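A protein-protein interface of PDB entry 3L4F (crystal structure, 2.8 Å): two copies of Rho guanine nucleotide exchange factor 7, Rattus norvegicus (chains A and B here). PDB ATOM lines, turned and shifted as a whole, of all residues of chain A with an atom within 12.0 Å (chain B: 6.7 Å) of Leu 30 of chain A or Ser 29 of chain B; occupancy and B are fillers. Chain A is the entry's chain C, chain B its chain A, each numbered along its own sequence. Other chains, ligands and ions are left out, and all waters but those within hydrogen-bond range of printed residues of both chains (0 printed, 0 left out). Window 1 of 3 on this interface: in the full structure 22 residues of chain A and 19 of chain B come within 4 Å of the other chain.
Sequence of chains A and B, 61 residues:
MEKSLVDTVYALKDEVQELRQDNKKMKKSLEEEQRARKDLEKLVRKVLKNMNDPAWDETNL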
ATOM      1  N   GLN A  21      -3.531  -7.338 -17.772  1.00  0.00           N
ATOM      2  CA  GLN A  21      -3.689  -7.811 -16.407  1.00  0.00           C
ATOM      3  C   GLN A  21      -3.227  -9.257 -16.324  1.00  0.00           C
ATOM      4  O   GLN A  21      -2.563  -9.650 -15.361  1.00  0.00           O
ATOM      5  CB  GLN A  21      -5.150  -7.669 -15.969  1.00  0.00           C
ATOM      6  CG  GLN A  21      -5.677  -6.246 -16.155  1.00  0.00           C
ATOM      7  CD  GLN A  21      -7.093  -6.057 -15.662  1.00  0.00           C
ATOM      8  OE1 GLN A  21      -7.962  -6.905 -15.877  1.00  0.00           O
ATOM      9  NE2 GLN A  21      -7.340  -4.924 -15.010  1.00  0.00           N
ATOM     10  N   ASP A  22      -3.554 -10.032 -17.356  1.00  0.00           N
ATOM     11  CA  ASP A  22      -3.171 -11.445 -17.429  1.00  0.00           C
ATOM     12  C   ASP A  22      -1.668 -11.680 -17.460  1.00  0.00           C
ATOM     13  O   ASP A  22      -1.155 -12.480 -16.677  1.00  0.00           O
ATOM     14  CB  ASP A  22      -3.787 -12.109 -18.660  1.00  0.00           C
ATOM     15  CG  ASP A  22      -4.978 -12.970 -18.316  1.00  0.00           C
ATOM     16  OD1 ASP A  22      -4.794 -13.952 -17.561  1.00  0.00           O
ATOM     17  OD2 ASP A  22      -6.093 -12.666 -18.800  1.00  0.00           O
ATOM     18  N   ASN A  23      -0.972 -11.005 -18.377  1.00  0.00           N
ATOM     19  CA  ASN A  23       0.477 -11.136 -18.501  1.00  0.00           C
ATOM     20  C   ASN A  23       1.097 -10.983 -17.126  1.00  0.00           C
ATOM     21  O   ASN A  23       2.109 -11.606 -16.823  1.00  0.00           O
ATOM     22  CB  ASN A  23       1.048 -10.059 -19.438  1.00  0.00           C
ATOM     23  CG  ASN A  23       0.702 -10.297 -20.904  1.00  0.00           C
ATOM     24  OD1 ASN A  23      -0.356 -10.832 -21.231  1.00  0.00           O
ATOM     25  ND2 ASN A  23       1.592  -9.878 -21.792  1.00  0.00           N
ATOM     26  N   LYS A  24       0.490 -10.156 -16.287  1.00  0.00           N
ATOM     27  CA  LYS A  24       1.016  -9.942 -14.945  1.00  0.00           C
ATOM     28  C   LYS A  24       0.867 -11.192 -14.065  1.00  0.00           C
ATOM     29  O   LYS A  24       1.794 -11.563 -13.342  1.00  0.00           O
ATOM     30  CB  LYS A  24       0.311  -8.741 -14.298  1.00  0.00           C
ATOM     31  CG  LYS A  24       0.524  -7.428 -15.047  1.00  0.00           C
ATOM     32  CD  LYS A  24      -0.354  -6.311 -14.503  1.00  0.00           C
ATOM     33  CE  LYS A  24      -0.286  -5.079 -15.397  1.00  0.00           C
ATOM     34  NZ  LYS A  24      -1.271  -4.032 -15.005  1.00  0.00           N
ATOM     35  N   LYS A  25      -0.300 -11.833 -14.128  1.00  0.00           N
ATOM     36  CA  LYS A  25      -0.559 -13.030 -13.334  1.00  0.00           C
ATOM     37  C   LYS A  25       0.287 -14.221 -13.814  1.00  0.00           C
ATOM     38  O   LYS A  25       0.746 -15.060 -13.013  1.00  0.00           O
ATOM     39  CB  LYS A  25      -2.048 -13.381 -13.398  1.00  0.00           C
ATOM     40  CG  LYS A  25      -2.969 -12.378 -12.692  1.00  0.00           C
ATOM     41  CD  LYS A  25      -4.407 -12.892 -12.548  1.00  0.00           C
ATOM     42  CE  LYS A  25      -5.096 -13.064 -13.895  1.00  0.00           C
ATOM     43  NZ  LYS A  25      -6.493 -13.577 -13.767  1.00  0.00           N
ATOM     44  N   MET A  26       0.482 -14.289 -15.128  1.00  0.00           N
ATOM     45  CA  MET A  26       1.270 -15.349 -15.729  1.00  0.00           C
ATOM     46  C   MET A  26       2.743 -15.120 -15.449  1.00  0.00           C
ATOM     47  O   MET A  26       3.480 -16.054 -15.130  1.00  0.00           O
ATOM     48  CB  MET A  26       1.035 -15.406 -17.240  1.00  0.00           C
ATOM     49  CG  MET A  26      -0.339 -15.946 -17.642  1.00  0.00           C
ATOM     50  SD  MET A  26      -0.402 -16.545 -19.363  1.00  0.00           S
ATOM     51  CE  MET A  26      -1.071 -15.146 -20.196  1.00  0.00           C
ATOM     52  N   LYS A  27       3.165 -13.866 -15.572  1.00  0.00           N
ATOM     53  CA  LYS A  27       4.553 -13.495 -15.330  1.00  0.00           C
ATOM     54  C   LYS A  27       4.835 -13.777 -13.872  1.00  0.00           C
ATOM     55  O   LYS A  27       5.951 -14.113 -13.490  1.00  0.00           O
ATOM     56  CB  LYS A  27       4.763 -12.003 -15.627  1.00  0.00           C
ATOM     57  CG  LYS A  27       6.221 -11.567 -15.691  1.00  0.00           C
ATOM     58  CD  LYS A  27       6.340 -10.177 -16.268  1.00  0.00           C
ATOM     59  CE  LYS A  27       7.722  -9.620 -16.060  1.00  0.00           C
ATOM     60  NZ  LYS A  27       7.804  -8.218 -16.547  1.00  0.00           N
ATOM     61  N   LYS A  28       3.785 -13.660 -13.068  1.00  0.00           N
ATOM     62  CA  LYS A  28       3.864 -13.882 -11.638  1.00  0.00           C
ATOM     63  C   LYS A  28       4.084 -15.365 -11.438  1.00  0.00           C
ATOM     64  O   LYS A  28       5.059 -15.781 -10.802  1.00  0.00           O
ATOM     65  CB  LYS A  28       2.555 -13.442 -10.964  1.00  0.00           C
ATOM     66  CG  LYS A  28       2.630 -13.380  -9.442  1.00  0.00           C
ATOM     67  CD  LYS A  28       1.257 -13.185  -8.827  1.00  0.00           C
ATOM     68  CE  LYS A  28       1.374 -12.960  -7.333  1.00  0.00           C
ATOM     69  NZ  LYS A  28       2.251 -13.973  -6.689  1.00  0.00           N
ATOM     70  N   SER A  29       3.175 -16.149 -12.017  1.00  0.00           N
ATOM     71  CA  SER A  29       3.219 -17.603 -11.932  1.00  0.00           C
ATOM     72  C   SER A  29       4.521 -18.168 -12.487  1.00  0.00           C
ATOM     73  O   SER A  29       5.205 -18.928 -11.807  1.00  0.00           O
ATOM     74  CB  SER A  29       2.029 -18.201 -12.676  1.00  0.00           C
ATOM     75  OG  SER A  29       0.818 -17.698 -12.141  1.00  0.00           O
ATOM     76  N   LEU A  30       4.856 -17.806 -13.720  1.00  0.00           N
ATOM     77  CA  LEU A  30       6.098 -18.264 -14.337  1.00  0.00           C
ATOM     78  C   LEU A  30       7.249 -18.202 -13.315  1.00  0.00           C
ATOM     79  O   LEU A  30       7.989 -19.179 -13.117  1.00  0.00           O
ATOM     80  CB  LEU A  30       6.451 -17.371 -15.532  1.00  0.00           C
ATOM     81  CG  LEU A  30       7.327 -17.992 -16.621  1.00  0.00           C
ATOM     82  CD1 LEU A  30       8.094 -16.907 -17.336  1.00  0.00           C
ATOM     83  CD2 LEU A  30       8.294 -18.974 -16.026  1.00  0.00           C
ATOM     84  N   GLU A  31       7.386 -17.048 -12.664  1.00  0.00           N
ATOM     85  CA  GLU A  31       8.448 -16.833 -11.682  1.00  0.00           C
ATOM     86  C   GLU A  31       8.291 -17.725 -10.454  1.00  0.00           C
ATOM     87  O   GLU A  31       9.269 -18.144  -9.842  1.00  0.00           O
ATOM     88  CB  GLU A  31       8.478 -15.361 -11.253  1.00  0.00           C
ATOM     89  CG  GLU A  31       8.689 -14.362 -12.393  1.00  0.00           C
ATOM     90  CD  GLU A  31       8.727 -12.913 -11.920  1.00  0.00           C
ATOM     91  OE1 GLU A  31       9.679 -12.542 -11.203  1.00  0.00           O
ATOM     92  OE2 GLU A  31       7.809 -12.142 -12.265  1.00  0.00           O
ATOM     93  N   GLU A  32       7.050 -18.014 -10.093  1.00  0.00           N
ATOM     94  CA  GLU A  32       6.783 -18.875  -8.950  1.00  0.00           C
ATOM     95  C   GLU A  32       7.179 -20.313  -9.281  1.00  0.00           C
ATOM     96  O   GLU A  32       7.688 -21.032  -8.425  1.00  0.00           O
ATOM     97  CB  GLU A  32       5.304 -18.780  -8.563  1.00  0.00           C
ATOM     98  CG  GLU A  32       4.943 -17.422  -7.949  1.00  0.00           C
ATOM     99  CD  GLU A  32       3.447 -17.149  -7.912  1.00  0.00           C
ATOM    100  OE1 GLU A  32       2.691 -18.001  -7.400  1.00  0.00           O
ATOM    101  OE2 GLU A  32       3.027 -16.074  -8.389  1.00  0.00           O
ATOM    102  N   GLU A  33       6.954 -20.712 -10.532  1.00  0.00           N
ATOM    103  CA  GLU A  33       7.299 -22.047 -11.025  1.00  0.00           C
ATOM    104  C   GLU A  33       8.808 -22.191 -10.959  1.00  0.00           C
ATOM    105  O   GLU A  33       9.334 -23.158 -10.389  1.00  0.00           O
ATOM    106  CB  GLU A  33       6.816 -22.187 -12.472  1.00  0.00           C
ATOM    107  CG  GLU A  33       7.243 -23.431 -13.225  1.00  0.00           C
ATOM    108  CD  GLU A  33       6.899 -24.714 -12.513  1.00  0.00           C
ATOM    109  OE1 GLU A  33       5.933 -24.727 -11.715  1.00  0.00           O
ATOM    110  OE2 GLU A  33       7.603 -25.717 -12.768  1.00  0.00           O
ATOM    111  N   GLN A  34       9.487 -21.194 -11.529  1.00  0.00           N
ATOM    112  CA  GLN A  34      10.946 -21.134 -11.579  1.00  0.00           C
ATOM    113  C   GLN A  34      11.599 -21.290 -10.213  1.00  0.00           C
ATOM    114  O   GLN A  34      12.744 -21.740 -10.115  1.00  0.00           O
ATOM    115  CB  GLN A  34      11.386 -19.814 -12.224  1.00  0.00           C
ATOM    116  CG  GLN A  34      12.890 -19.605 -12.311  1.00  0.00           C
ATOM    117  CD  GLN A  34      13.262 -18.374 -13.127  1.00  0.00           C
ATOM    118  OE1 GLN A  34      14.395 -17.875 -13.052  1.00  0.00           O
ATOM    119  NE2 GLN A  34      12.311 -17.886 -13.923  1.00  0.00           N
ATOM    120  N   ARG A  35      10.882 -20.917  -9.157  1.00  0.00           N
ATOM    121  CA  ARG A  35      11.439 -21.062  -7.816  1.00  0.00           C
ATOM    122  C   ARG A  35      11.234 -22.492  -7.362  1.00  0.00           C
ATOM    123  O   ARG A  35      12.120 -23.086  -6.748  1.00  0.00           O
ATOM    124  CB  ARG A  35      10.763 -20.113  -6.830  1.00  0.00           C
ATOM    125  CG  ARG A  35      11.702 -19.564  -5.774  1.00  0.00           C
ATOM    126  CD  ARG A  35      11.043 -18.394  -5.109  1.00  0.00           C
ATOM    127  NE  ARG A  35      10.703 -17.344  -6.069  1.00  0.00           N
ATOM    128  CZ  ARG A  35       9.575 -16.637  -6.046  1.00  0.00           C
ATOM    129  NH1 ARG A  35       8.658 -16.864  -5.112  1.00  0.00           N
ATOM    130  NH2 ARG A  35       9.368 -15.692  -6.954  1.00  0.00           N
ATOM    131  N   ALA A  36      10.069 -23.047  -7.681  1.00  0.00           N
ATOM    132  CA  ALA A  36       9.762 -24.417  -7.311  1.00  0.00           C
ATOM    133  C   ALA A  36      10.663 -25.358  -8.100  1.00  0.00           C
ATOM    134  O   ALA A  36      11.203 -26.311  -7.548  1.00  0.00           O
ATOM    135  CB  ALA A  36       8.312 -24.723  -7.586  1.00  0.00           C
ATOM    136  N   ARG A  37      10.826 -25.089  -9.387  1.00  0.00           N
ATOM    137  CA  ARG A  37      11.700 -25.913 -10.218  1.00  0.00           C
ATOM    138  C   ARG A  37      13.063 -26.003  -9.537  1.00  0.00           C
ATOM    139  O   ARG A  37      13.516 -27.087  -9.172  1.00  0.00           O
ATOM    140  CB  ARG A  37      11.877 -25.282 -11.601  1.00  0.00           C
ATOM    141  CG  ARG A  37      12.664 -26.138 -12.592  1.00  0.00           C
ATOM    142  CD  ARG A  37      13.370 -25.269 -13.619  1.00  0.00           C
ATOM    143  NE  ARG A  37      14.597 -24.705 -13.061  1.00  0.00           N
ATOM    144  CZ  ARG A  37      15.268 -23.688 -13.591  1.00  0.00           C
ATOM    145  NH1 ARG A  37      14.828 -23.105 -14.697  1.00  0.00           N
ATOM    146  NH2 ARG A  37      16.395 -23.272 -13.028  1.00  0.00           N
ATOM    147  N   LYS A  38      13.707 -24.850  -9.364  1.00  0.00           N
ATOM    148  CA  LYS A  38      15.023 -24.788  -8.740  1.00  0.00           C
ATOM    149  C   LYS A  38      15.042 -25.413  -7.333  1.00  0.00           C
ATOM    150  O   LYS A  38      15.998 -26.121  -6.968  1.00  0.00           O
ATOM    151  CB  LYS A  38      15.515 -23.333  -8.722  1.00  0.00           C
ATOM    152  CG  LYS A  38      15.877 -22.816 -10.115  1.00  0.00           C
ATOM    153  CD  LYS A  38      16.057 -21.300 -10.190  1.00  0.00           C
ATOM    154  CE  LYS A  38      16.401 -20.892 -11.626  1.00  0.00           C
ATOM    155  NZ  LYS A  38      16.375 -19.430 -11.894  1.00  0.00           N
ATOM    156  N   ASP A  39      13.988 -25.179  -6.553  1.00  0.00           N
ATOM    157  CA  ASP A  39      13.937 -25.757  -5.216  1.00  0.00           C
ATOM    158  C   ASP A  39      14.067 -27.253  -5.405  1.00  0.00           C
ATOM    159  O   ASP A  39      14.822 -27.902  -4.685  1.00  0.00           O
ATOM    160  CB  ASP A  39      12.616 -25.448  -4.486  1.00  0.00           C
ATOM    161  CG  ASP A  39      12.521 -24.012  -4.026  1.00  0.00           C
ATOM    162  OD1 ASP A  39      13.541 -23.467  -3.554  1.00  0.00           O
ATOM    163  OD2 ASP A  39      11.419 -23.429  -4.123  1.00  0.00           O
ATOM    164  N   ASN B  23       4.865 -10.377 -24.727  1.00  0.00           N
ATOM    165  CA  ASN B  23       4.640 -11.746 -25.159  1.00  0.00           C
ATOM    166  C   ASN B  23       5.901 -12.433 -25.694  1.00  0.00           C
ATOM    167  O   ASN B  23       6.219 -13.553 -25.280  1.00  0.00           O
ATOM    168  CB  ASN B  23       3.505 -11.790 -26.186  1.00  0.00           C
ATOM    169  CG  ASN B  23       2.142 -11.998 -25.533  1.00  0.00           C
ATOM    170  OD1 ASN B  23       1.991 -11.813 -24.323  1.00  0.00           O
ATOM    171  ND2 ASN B  23       1.145 -12.380 -26.331  1.00  0.00           N
ATOM    172  N   LYS B  24       6.629 -11.767 -26.589  1.00  0.00           N
ATOM    173  CA  LYS B  24       7.851 -12.351 -27.128  1.00  0.00           C
ATOM    174  C   LYS B  24       8.807 -12.652 -25.986  1.00  0.00           C
ATOM    175  O   LYS B  24       9.606 -13.585 -26.058  1.00  0.00           O
ATOM    176  CB  LYS B  24       8.468 -11.409 -28.158  1.00  0.00           C
ATOM    177  CG  LYS B  24       7.730 -11.472 -29.493  1.00  0.00           C
ATOM    178  CD  LYS B  24       7.965 -10.260 -30.379  1.00  0.00           C
ATOM    179  CE  LYS B  24       6.966 -10.241 -31.535  1.00  0.00           C
ATOM    180  NZ  LYS B  24       6.939  -8.934 -32.243  1.00  0.00           N
ATOM    181  N   LYS B  25       8.710 -11.864 -24.922  1.00  0.00           N
ATOM    182  CA  LYS B  25       9.530 -12.095 -23.741  1.00  0.00           C
ATOM    183  C   LYS B  25       8.941 -13.291 -22.979  1.00  0.00           C
ATOM    184  O   LYS B  25       9.668 -14.224 -22.620  1.00  0.00           O
ATOM    185  CB  LYS B  25       9.561 -10.844 -22.857  1.00  0.00           C
ATOM    186  CG  LYS B  25      10.346  -9.705 -23.480  1.00  0.00           C
ATOM    187  CD  LYS B  25      10.526  -8.519 -22.538  1.00  0.00           C
ATOM    188  CE  LYS B  25      11.463  -7.476 -23.173  1.00  0.00           C
ATOM    189  NZ  LYS B  25      11.740  -6.263 -22.342  1.00  0.00           N
ATOM    190  N   MET B  26       7.624 -13.264 -22.757  1.00  0.00           N
ATOM    191  CA  MET B  26       6.914 -14.347 -22.069  1.00  0.00           C
ATOM    192  C   MET B  26       7.208 -15.689 -22.723  1.00  0.00           C
ATOM    193  O   MET B  26       7.643 -16.617 -22.049  1.00  0.00           O
ATOM    194  CB  MET B  26       5.407 -14.112 -22.114  1.00  0.00           C
ATOM    195  CG  MET B  26       4.897 -12.973 -21.241  1.00  0.00           C
ATOM    196  SD  MET B  26       4.837 -13.385 -19.484  1.00  0.00           S
ATOM    197  CE  MET B  26       4.473 -15.191 -19.543  1.00  0.00           C
ATOM    198  N   LYS B  27       6.965 -15.780 -24.034  1.00  0.00           N
ATOM    199  CA  LYS B  27       7.189 -17.013 -24.800  1.00  0.00           C
ATOM    200  C   LYS B  27       8.619 -17.505 -24.685  1.00  0.00           C
ATOM    201  O   LYS B  27       8.865 -18.710 -24.654  1.00  0.00           O
ATOM    202  CB  LYS B  27       6.861 -16.804 -26.285  1.00  0.00           C
ATOM    203  CG  LYS B  27       6.966 -18.067 -27.123  1.00  0.00           C
ATOM    204  CD  LYS B  27       5.664 -18.387 -27.863  1.00  0.00           C
ATOM    205  CE  LYS B  27       5.763 -19.736 -28.588  1.00  0.00           C
ATOM    206  NZ  LYS B  27       4.538 -20.096 -29.359  1.00  0.00           N
ATOM    207  N   LYS B  28       9.558 -16.567 -24.607  1.00  0.00           N
ATOM    208  CA  LYS B  28      10.965 -16.906 -24.516  1.00  0.00           C
ATOM    209  C   LYS B  28      11.272 -17.450 -23.140  1.00  0.00           C
ATOM    210  O   LYS B  28      12.133 -18.313 -22.983  1.00  0.00           O
ATOM    211  CB  LYS B  28      11.815 -15.670 -24.774  1.00  0.00           C
ATOM    212  CG  LYS B  28      13.211 -15.943 -25.275  1.00  0.00           C
ATOM    213  CD  LYS B  28      13.299 -15.754 -26.778  1.00  0.00           C
ATOM    214  CE  LYS B  28      12.979 -14.314 -27.173  1.00  0.00           C
ATOM    215  NZ  LYS B  28      13.113 -14.100 -28.644  1.00  0.00           N
ATOM    216  N   SER B  29      10.571 -16.950 -22.133  1.00  0.00           N
ATOM    217  CA  SER B  29      10.809 -17.430 -20.783  1.00  0.00           C
ATOM    218  C   SER B  29      10.328 -18.854 -20.576  1.00  0.00           C
ATOM    219  O   SER B  29      11.072 -19.661 -20.035  1.00  0.00           O
ATOM    220  CB  SER B  29      10.174 -16.501 -19.755  1.00  0.00           C
ATOM    221  OG  SER B  29      10.939 -15.313 -19.634  1.00  0.00           O
ATOM    222  N   LEU B  30       9.100 -19.180 -20.986  1.00  0.00           N
ATOM    223  CA  LEU B  30       8.628 -20.554 -20.825  1.00  0.00           C
ATOM    224  C   LEU B  30       9.610 -21.476 -21.542  1.00  0.00           C
ATOM    225  O   LEU B  30      10.050 -22.495 -20.997  1.00  0.00           O
ATOM    226  CB  LEU B  30       7.229 -20.734 -21.399  1.00  0.00           C
ATOM    227  CG  LEU B  30       6.104 -20.418 -20.426  1.00  0.00           C
ATOM    228  CD1 LEU B  30       5.912 -18.913 -20.374  1.00  0.00           C
ATOM    229  CD2 LEU B  30       4.827 -21.114 -20.871  1.00  0.00           C
ATOM    230  N   GLU B  31       9.962 -21.113 -22.771  1.00  0.00           N
ATOM    231  CA  GLU B  31      10.942 -21.899 -23.516  1.00  0.00           C
ATOM    232  C   GLU B  31      12.148 -22.240 -22.614  1.00  0.00           C
ATOM    233  O   GLU B  31      12.443 -23.421 -22.396  1.00  0.00           O
ATOM    234  CB  GLU B  31      11.425 -21.129 -24.743  1.00  0.00           C
ATOM    235  CG  GLU B  31      10.494 -21.215 -25.933  1.00  0.00           C
ATOM    236  CD  GLU B  31      11.027 -20.455 -27.135  1.00  0.00           C
ATOM    237  OE1 GLU B  31      12.230 -20.624 -27.452  1.00  0.00           O
ATOM    238  OE2 GLU B  31      10.247 -19.698 -27.762  1.00  0.00           O
ATOM    239  N   GLU B  32      12.825 -21.212 -22.089  1.00  0.00           N
ATOM    240  CA  GLU B  32      13.971 -21.431 -21.205  1.00  0.00           C
ATOM    241  C   GLU B  32      13.540 -22.306 -20.038  1.00  0.00           C
ATOM    242  O   GLU B  32      14.198 -23.291 -19.702  1.00  0.00           O
ATOM    243  CB  GLU B  32      14.500 -20.106 -20.670  1.00  0.00           C
ATOM    244  CG  GLU B  32      14.739 -19.085 -21.765  1.00  0.00           C
ATOM    245  CD  GLU B  32      15.139 -17.729 -21.224  1.00  0.00           C
ATOM    246  OE1 GLU B  32      16.209 -17.644 -20.589  1.00  0.00           O
ATOM    247  OE2 GLU B  32      14.382 -16.752 -21.434  1.00  0.00           O
ATOM    248  N   GLU B  33      12.417 -21.946 -19.435  1.00  0.00           N
ATOM    249  CA  GLU B  33      11.891 -22.704 -18.310  1.00  0.00           C
ATOM    250  C   GLU B  33      11.746 -24.175 -18.684  1.00  0.00           C
ATOM    251  O   GLU B  33      12.076 -25.055 -17.896  1.00  0.00           O
ATOM    252  CB  GLU B  33      10.534 -22.157 -17.887  1.00  0.00           C
ATOM    253  CG  GLU B  33      10.098 -22.706 -16.564  1.00  0.00           C
ATOM    254  CD  GLU B  33      11.194 -22.597 -15.523  1.00  0.00           C
ATOM    255  OE1 GLU B  33      11.765 -21.493 -15.359  1.00  0.00           O
ATOM    256  OE2 GLU B  33      11.482 -23.618 -14.867  1.00  0.00           O
ATOM    257  N   GLN B  34      11.245 -24.435 -19.887  1.00  0.00           N
ATOM    258  CA  GLN B  34      11.084 -25.805 -20.348  1.00  0.00           C
ATOM    259  C   GLN B  34      12.438 -26.515 -20.509  1.00  0.00           C
ATOM    260  O   GLN B  34      12.595 -27.620 -19.993  1.00  0.00           O
ATOM    261  CB  GLN B  34      10.310 -25.840 -21.666  1.00  0.00           C
ATOM    262  CG  GLN B  34       8.873 -25.399 -21.568  1.00  0.00           C
ATOM    263  CD  GLN B  34       8.237 -25.245 -22.937  1.00  0.00           C
ATOM    264  OE1 GLN B  34       8.207 -26.190 -23.734  1.00  0.00           O
ATOM    265  NE2 GLN B  34       7.727 -24.049 -23.220  1.00  0.00           N
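The side-chain amide oxygen (OD1) of Asn 23 of chain B sits at hydrogen-bond distance from the side-chain amide nitrogen (ND2) of Asn 23 of chain A, 3.2 Å away. NH1 of Arg 37 of chain A is in salt-bridge range of OE2 of Glu 33 of chain B, 3.4 Å away.
OG of Ser 29 of chain B lies within hydrogen-bond range of O of Lys 25 of chain B (3.4 Å). The side-chain amino group (NZ) of Lys 38 of chain A sits at hydrogen-bond distance from the side-chain amide oxygen (OE1) of Gln 34 of chain A, at 2.8 Å.
Among the printed residues, merely in contact across the chains: Leu 30 of chain A with Ser 29 of chain B (3.2 Å) and Gln 34 of chain A with Glu 33 of chain B (3.6 Å).
Printed residues of chain B within 4 Å of Asn 23 of chain A: Asn 23. Of chain B, only Ser 29 (3.2 Å) comes within 4 Å of Leu 30 of chain A. Printed residues of chain B within 4 Å of Gln 34 of chain A: Glu 33 (3.6 Å). Printed residues of chain B within 4 Å of Arg 37 of chain A: Glu 33 (2.8 Å). Of the printed residues of chain A, Asn 23 of chain B touches Asn 23 (3.2 Å). Met 26 of chain B touches none of the printed residues of chain A. Ser 29 of chain B touches just one residue of chain A: Leu 30 (3.2 Å). No residue of chain A comes within 4 Å of Leu 30 of chain B. No residue of chain A comes within 4 Å of Glu 31 of chain B. Glu 33 of chain B touches two residues of chain A.
Along chain B the printed residues that touch a printed residue of chain A span positions 23 to 33. Among the printed residues, Asp or Glu carboxylates within 4 Å of a Lys or Arg side-chain nitrogen of the other chain: Arg 37 of chain A with Glu 33 of chain B.
Asn 23 of chain A touches its own counterpart, Asn 23 of chain B. Leu 30 of chain A touches Ser 29 of chain B, but with the chains exchanged Ser 29 of chain A does not touch Leu 30 of chain B (8.0 Å). Gln 34 of chain A touches Glu 33 of chain B, but with the chains exchanged Glu 33 of chain A does not touch Gln 34 of chain B (7.8 Å). Positions printed for both chains: 23, 24, 25, 26, 27, 28, 29, 30, 31, 32, 33 and 34. Of the 4 pairs that touch across the chains among the printed residues, 1 has its exchanged pair printed and touching as well.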
